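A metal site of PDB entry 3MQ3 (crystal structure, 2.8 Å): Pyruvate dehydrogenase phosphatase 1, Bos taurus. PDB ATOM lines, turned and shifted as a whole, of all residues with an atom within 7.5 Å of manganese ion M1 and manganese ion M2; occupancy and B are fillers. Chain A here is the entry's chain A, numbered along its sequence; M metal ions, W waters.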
ATOM      1  N   ASN A  49      36.135 -14.183  30.443  1.00  0.00           N
ATOM      2  CA  ASN A  49      36.292 -15.609  30.179  1.00  0.00           C
ATOM      3  C   ASN A  49      37.492 -15.891  29.271  1.00  0.00           C
ATOM      4  O   ASN A  49      38.004 -14.992  28.603  1.00  0.00           O
ATOM      5  CB  ASN A  49      35.016 -16.191  29.553  1.00  0.00           C
ATOM      6  CG  ASN A  49      33.928 -16.427  30.576  1.00  0.00           C
ATOM      7  OD1 ASN A  49      32.832 -15.897  30.460  1.00  0.00           O
ATOM      8  ND2 ASN A  49      34.235 -17.228  31.587  1.00  0.00           N
ATOM      9  N   ILE A  52      36.794 -15.075  24.974  1.00  0.00           N
ATOM     10  CA  ILE A  52      35.602 -14.283  25.322  1.00  0.00           C
ATOM     11  C   ILE A  52      34.334 -14.987  24.848  1.00  0.00           C
ATOM     12  O   ILE A  52      34.323 -15.571  23.779  1.00  0.00           O
ATOM     13  CB  ILE A  52      35.642 -12.790  24.811  1.00  0.00           C
ATOM     14  CG1 ILE A  52      34.483 -11.978  25.447  1.00  0.00           C
ATOM     15  CG2 ILE A  52      35.620 -12.716  23.307  1.00  0.00           C
ATOM     16  CD1 ILE A  52      34.793 -10.470  25.734  1.00  0.00           C
ATOM     17  N   GLU A  53      33.280 -14.933  25.634  1.00  0.00           N
ATOM     18  CA  GLU A  53      32.026 -15.575  25.196  1.00  0.00           C
ATOM     19  C   GLU A  53      30.889 -14.677  24.545  1.00  0.00           C
ATOM     20  O   GLU A  53      29.978 -15.191  23.857  1.00  0.00           O
ATOM     21  CB  GLU A  53      31.517 -16.486  26.283  1.00  0.00           C
ATOM     22  CG  GLU A  53      32.312 -17.747  26.302  1.00  0.00           C
ATOM     23  CD  GLU A  53      31.862 -18.752  27.349  1.00  0.00           C
ATOM     24  OE1 GLU A  53      30.836 -18.546  28.039  1.00  0.00           O
ATOM     25  OE2 GLU A  53      32.569 -19.758  27.485  1.00  0.00           O
ATOM     26  N   ASP A  54      31.044 -13.346  24.732  1.00  0.00           N
ATOM     27  CA  ASP A  54      30.240 -12.329  24.071  1.00  0.00           C
ATOM     28  C   ASP A  54      30.668 -12.199  22.629  1.00  0.00           C
ATOM     29  O   ASP A  54      31.749 -12.576  22.287  1.00  0.00           O
ATOM     30  CB  ASP A  54      30.442 -10.984  24.740  1.00  0.00           C
ATOM     31  CG  ASP A  54      29.665 -10.825  26.018  1.00  0.00           C
ATOM     32  OD1 ASP A  54      29.031 -11.779  26.519  1.00  0.00           O
ATOM     33  OD2 ASP A  54      29.700  -9.688  26.550  1.00  0.00           O
ATOM     34  N   PHE A  72      25.621 -10.406  21.539  1.00  0.00           N
ATOM     35  CA  PHE A  72      25.259 -11.827  21.728  1.00  0.00           C
ATOM     36  C   PHE A  72      26.085 -12.341  22.869  1.00  0.00           C
ATOM     37  O   PHE A  72      27.286 -12.120  22.930  1.00  0.00           O
ATOM     38  CB  PHE A  72      25.585 -12.635  20.462  1.00  0.00           C
ATOM     39  CG  PHE A  72      25.107 -12.001  19.193  1.00  0.00           C
ATOM     40  CD1 PHE A  72      25.887 -11.013  18.539  1.00  0.00           C
ATOM     41  CD2 PHE A  72      23.881 -12.348  18.643  1.00  0.00           C
ATOM     42  CE1 PHE A  72      25.487 -10.402  17.362  1.00  0.00           C
ATOM     43  CE2 PHE A  72      23.465 -11.724  17.427  1.00  0.00           C
ATOM     44  CZ  PHE A  72      24.269 -10.768  16.793  1.00  0.00           C
ATOM     45  N   ASP A  73      25.441 -12.977  23.813  1.00  0.00           N
ATOM     46  CA  ASP A  73      26.136 -13.402  25.012  1.00  0.00           C
ATOM     47  C   ASP A  73      26.071 -14.903  25.033  1.00  0.00           C
ATOM     48  O   ASP A  73      25.015 -15.479  25.359  1.00  0.00           O
ATOM     49  CB  ASP A  73      25.469 -12.803  26.231  1.00  0.00           C
ATOM     50  CG  ASP A  73      26.069 -13.284  27.560  1.00  0.00           C
ATOM     51  OD1 ASP A  73      25.709 -12.706  28.619  1.00  0.00           O
ATOM     52  OD2 ASP A  73      26.900 -14.233  27.566  1.00  0.00           O
ATOM     53  N   GLY A  74      27.196 -15.522  24.666  1.00  0.00           N
ATOM     54  CA  GLY A  74      27.428 -16.983  24.739  1.00  0.00           C
ATOM     55  C   GLY A  74      27.537 -17.521  26.155  1.00  0.00           C
ATOM     56  O   GLY A  74      27.913 -16.780  27.096  1.00  0.00           O
ATOM     57  N   HIS A  75      27.135 -18.772  26.307  1.00  0.00           N
ATOM     58  CA  HIS A  75      27.307 -19.540  27.531  1.00  0.00           C
ATOM     59  C   HIS A  75      27.659 -20.967  27.117  1.00  0.00           C
ATOM     60  O   HIS A  75      27.368 -21.373  25.955  1.00  0.00           O
ATOM     61  CB  HIS A  75      26.122 -19.446  28.495  1.00  0.00           C
ATOM     62  CG  HIS A  75      24.781 -19.722  27.874  1.00  0.00           C
ATOM     63  ND1 HIS A  75      24.312 -21.010  27.671  1.00  0.00           N
ATOM     64  CD2 HIS A  75      23.796 -18.889  27.455  1.00  0.00           C
ATOM     65  CE1 HIS A  75      23.105 -20.943  27.105  1.00  0.00           C
ATOM     66  NE2 HIS A  75      22.777 -19.674  26.968  1.00  0.00           N
ATOM     67  N   ALA A  76      28.359 -21.673  27.999  1.00  0.00           N
ATOM     68  CA  ALA A  76      28.803 -23.023  27.687  1.00  0.00           C
ATOM     69  C   ALA A  76      29.678 -23.061  26.412  1.00  0.00           C
ATOM     70  O   ALA A  76      29.518 -23.937  25.549  1.00  0.00           O
ATOM     71  CB  ALA A  76      27.620 -23.943  27.534  1.00  0.00           C
ATOM     72  N   GLY A  77      30.601 -22.110  26.295  1.00  0.00           N
ATOM     73  CA  GLY A  77      31.448 -21.994  25.125  1.00  0.00           C
ATOM     74  C   GLY A  77      31.054 -20.786  24.269  1.00  0.00           C
ATOM     75  O   GLY A  77      30.158 -20.033  24.642  1.00  0.00           O
ATOM     76  N   SER A  81      27.557 -18.215  20.084  1.00  0.00           N
ATOM     77  CA  SER A  81      27.543 -16.757  19.932  1.00  0.00           C
ATOM     78  C   SER A  81      28.329 -16.391  18.681  1.00  0.00           C
ATOM     79  O   SER A  81      27.908 -15.548  17.912  1.00  0.00           O
ATOM     80  CB  SER A  81      28.038 -16.015  21.181  1.00  0.00           C
ATOM     81  OG  SER A  81      29.286 -16.499  21.606  1.00  0.00           O
ATOM     82  N   GLY A 200      25.005 -22.153  23.954  1.00  0.00           N
ATOM     83  CA  GLY A 200      23.880 -21.227  23.770  1.00  0.00           C
ATOM     84  C   GLY A 200      24.296 -19.759  23.677  1.00  0.00           C
ATOM     85  O   GLY A 200      25.423 -19.393  24.040  1.00  0.00           O
ATOM     86  N   THR A 202      22.502 -15.611  23.745  1.00  0.00           N
ATOM     87  CA  THR A 202      21.524 -14.551  23.862  1.00  0.00           C
ATOM     88  C   THR A 202      21.616 -13.778  22.559  1.00  0.00           C
ATOM     89  O   THR A 202      22.612 -13.948  21.843  1.00  0.00           O
ATOM     90  CB  THR A 202      21.989 -13.667  25.045  1.00  0.00           C
ATOM     91  OG1 THR A 202      20.997 -13.621  26.066  1.00  0.00           O
ATOM     92  CG2 THR A 202      22.462 -12.247  24.623  1.00  0.00           C
ATOM     93  N   ASP A 220      18.924 -11.984  27.997  1.00  0.00           N
ATOM     94  CA  ASP A 220      19.038 -11.003  29.107  1.00  0.00           C
ATOM     95  C   ASP A 220      20.063  -9.938  28.786  1.00  0.00           C
ATOM     96  O   ASP A 220      20.626  -9.323  29.664  1.00  0.00           O
ATOM     97  CB  ASP A 220      19.322 -11.697  30.423  1.00  0.00           C
ATOM     98  CG  ASP A 220      20.490 -12.637  30.331  1.00  0.00           C
ATOM     99  OD1 ASP A 220      20.699 -13.416  31.273  1.00  0.00           O
ATOM    100  OD2 ASP A 220      21.246 -12.605  29.320  1.00  0.00           O
ATOM    101  N   SER A 221      20.307  -9.734  27.489  1.00  0.00           N
ATOM    102  CA  SER A 221      21.080  -8.602  27.009  1.00  0.00           C
ATOM    103  C   SER A 221      20.053  -7.514  26.786  1.00  0.00           C
ATOM    104  O   SER A 221      18.871  -7.766  26.884  1.00  0.00           O
ATOM    105  CB  SER A 221      21.833  -8.952  25.715  1.00  0.00           C
ATOM    106  OG  SER A 221      22.938  -9.812  25.960  1.00  0.00           O
ATOM    107  N   THR A 346      25.548  -6.495  26.630  1.00  0.00           N
ATOM    108  CA  THR A 346      25.321  -7.706  27.410  1.00  0.00           C
ATOM    109  C   THR A 346      25.233  -7.380  28.895  1.00  0.00           C
ATOM    110  O   THR A 346      25.360  -6.216  29.283  1.00  0.00           O
ATOM    111  CB  THR A 346      26.373  -8.751  27.132  1.00  0.00           C
ATOM    112  OG1 THR A 346      27.672  -8.222  27.401  1.00  0.00           O
ATOM    113  CG2 THR A 346      26.325  -9.164  25.692  1.00  0.00           C
ATOM    114  N   ASP A 347      24.934  -8.362  29.742  1.00  0.00           N
ATOM    115  CA  ASP A 347      24.590  -8.064  31.118  1.00  0.00           C
ATOM    116  C   ASP A 347      25.820  -7.721  31.958  1.00  0.00           C
ATOM    117  O   ASP A 347      25.700  -7.165  33.034  1.00  0.00           O
ATOM    118  CB  ASP A 347      23.780  -9.210  31.749  1.00  0.00           C
ATOM    119  CG  ASP A 347      24.448 -10.566  31.598  1.00  0.00           C
ATOM    120  OD1 ASP A 347      25.572 -10.659  30.988  1.00  0.00           O
ATOM    121  OD2 ASP A 347      23.798 -11.544  32.087  1.00  0.00           O
ATOM    122  N   GLY A 348      27.008  -8.037  31.443  1.00  0.00           N
ATOM    123  CA  GLY A 348      28.248  -7.577  32.041  1.00  0.00           C
ATOM    124  C   GLY A 348      28.266  -6.067  32.229  1.00  0.00           C
ATOM    125  O   GLY A 348      28.838  -5.570  33.194  1.00  0.00           O
ATOM    126  N   LEU A 349      27.642  -5.316  31.332  1.00  0.00           N
ATOM    127  CA  LEU A 349      27.426  -3.910  31.572  1.00  0.00           C
ATOM    128  C   LEU A 349      26.311  -3.755  32.554  1.00  0.00           C
ATOM    129  O   LEU A 349      26.514  -3.194  33.614  1.00  0.00           O
ATOM    130  CB  LEU A 349      27.058  -3.188  30.290  1.00  0.00           C
ATOM    131  CG  LEU A 349      26.823  -1.700  30.566  1.00  0.00           C
ATOM    132  CD1 LEU A 349      27.971  -1.050  31.384  1.00  0.00           C
ATOM    133  CD2 LEU A 349      26.525  -0.933  29.276  1.00  0.00           C
ATOM    134  N   GLU A 351      24.433  -5.544  34.844  1.00  0.00           N
ATOM    135  CA  GLU A 351      24.605  -5.932  36.270  1.00  0.00           C
ATOM    136  C   GLU A 351      25.448  -4.939  37.051  1.00  0.00           C
ATOM    137  O   GLU A 351      25.228  -4.766  38.206  1.00  0.00           O
ATOM    138  CB  GLU A 351      25.187  -7.333  36.426  1.00  0.00           C
ATOM    139  CG  GLU A 351      24.380  -8.417  35.717  1.00  0.00           C
ATOM    140  CD  GLU A 351      23.137  -8.970  36.459  1.00  0.00           C
ATOM    141  OE1 GLU A 351      22.189  -8.189  36.776  1.00  0.00           O
ATOM    142  OE2 GLU A 351      23.094 -10.221  36.665  1.00  0.00           O
ATOM    143  N   ASP A 445      31.792 -10.142  34.468  1.00  0.00           N
ATOM    144  CA  ASP A 445      31.396 -10.984  33.342  1.00  0.00           C
ATOM    145  C   ASP A 445      32.133 -10.430  32.125  1.00  0.00           C
ATOM    146  O   ASP A 445      32.811  -9.395  32.232  1.00  0.00           O
ATOM    147  CB  ASP A 445      29.873 -10.855  33.188  1.00  0.00           C
ATOM    148  CG  ASP A 445      29.262 -11.912  32.343  1.00  0.00           C
ATOM    149  OD1 ASP A 445      29.977 -12.742  31.793  1.00  0.00           O
ATOM    150  OD2 ASP A 445      28.035 -11.932  32.231  1.00  0.00           O
ATOM    151  N   ASP A 446      32.002 -11.101  30.983  1.00  0.00           N
ATOM    152  CA  ASP A 446      32.295 -10.461  29.680  1.00  0.00           C
ATOM    153  C   ASP A 446      31.447  -9.193  29.514  1.00  0.00           C
ATOM    154  O   ASP A 446      30.304  -9.166  29.926  1.00  0.00           O
ATOM    155  CB  ASP A 446      32.031 -11.431  28.524  1.00  0.00           C
ATOM    156  CG  ASP A 446      32.850 -12.720  28.629  1.00  0.00           C
ATOM    157  OD1 ASP A 446      33.938 -12.717  29.276  1.00  0.00           O
ATOM    158  OD2 ASP A 446      32.437 -13.733  28.038  1.00  0.00           O
ATOM    159  N   ILE A 447      32.019  -8.142  28.945  1.00  0.00           N
ATOM    160  CA  ILE A 447      31.306  -6.903  28.735  1.00  0.00           C
ATOM    161  C   ILE A 447      31.451  -6.579  27.275  1.00  0.00           C
ATOM    162  O   ILE A 447      32.584  -6.513  26.747  1.00  0.00           O
ATOM    163  CB  ILE A 447      31.883  -5.789  29.603  1.00  0.00           C
ATOM    164  CG1 ILE A 447      31.690  -6.155  31.077  1.00  0.00           C
ATOM    165  CG2 ILE A 447      31.192  -4.486  29.319  1.00  0.00           C
ATOM    166  CD1 ILE A 447      32.532  -5.314  32.054  1.00  0.00           C
HETATM  167 MN    MN M   1      26.844 -12.284  30.446  1.00  0.00          MN
HETATM  168 MN    MN M   2      28.177 -15.293  28.700  1.00  0.00          MN
HETATM  169  O   HOH W   1      25.604 -13.375  31.486  1.00  0.00           O
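The backbone carbonyl oxygen of Asp 73 lies within hydrogen-bond range of the backbone NH of Thr 202, at 3.0 Å. The backbone carbonyl oxygen (O) of Glu 53 is in hydrogen-bond range of the backbone NH (N) of Gly 74, at 2.9 Å.
Of the 23 residues printed, 3 come within 4 Å of manganese ion M1.
The nearest printed residue that does not touch manganese ion M2 is Asp 54 (4.2 Å).
Manganese ion M1 is bound by water W1 (2.0 Å), OD1 of Asp 347 (2.1 Å), OD2 of Asp 445 (2.2 Å) and OD1 of Asp 73 (2.2 Å).
Manganese ion M2 is bound by the side-chain carboxylate (OD2) of Asp 73 (2.0 Å). The backbone carbonyl oxygen (O) of Gly 74 is bound to manganese ion M2, 2.2 Å away. Manganese ion M2 has two donor atoms within binding distance.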
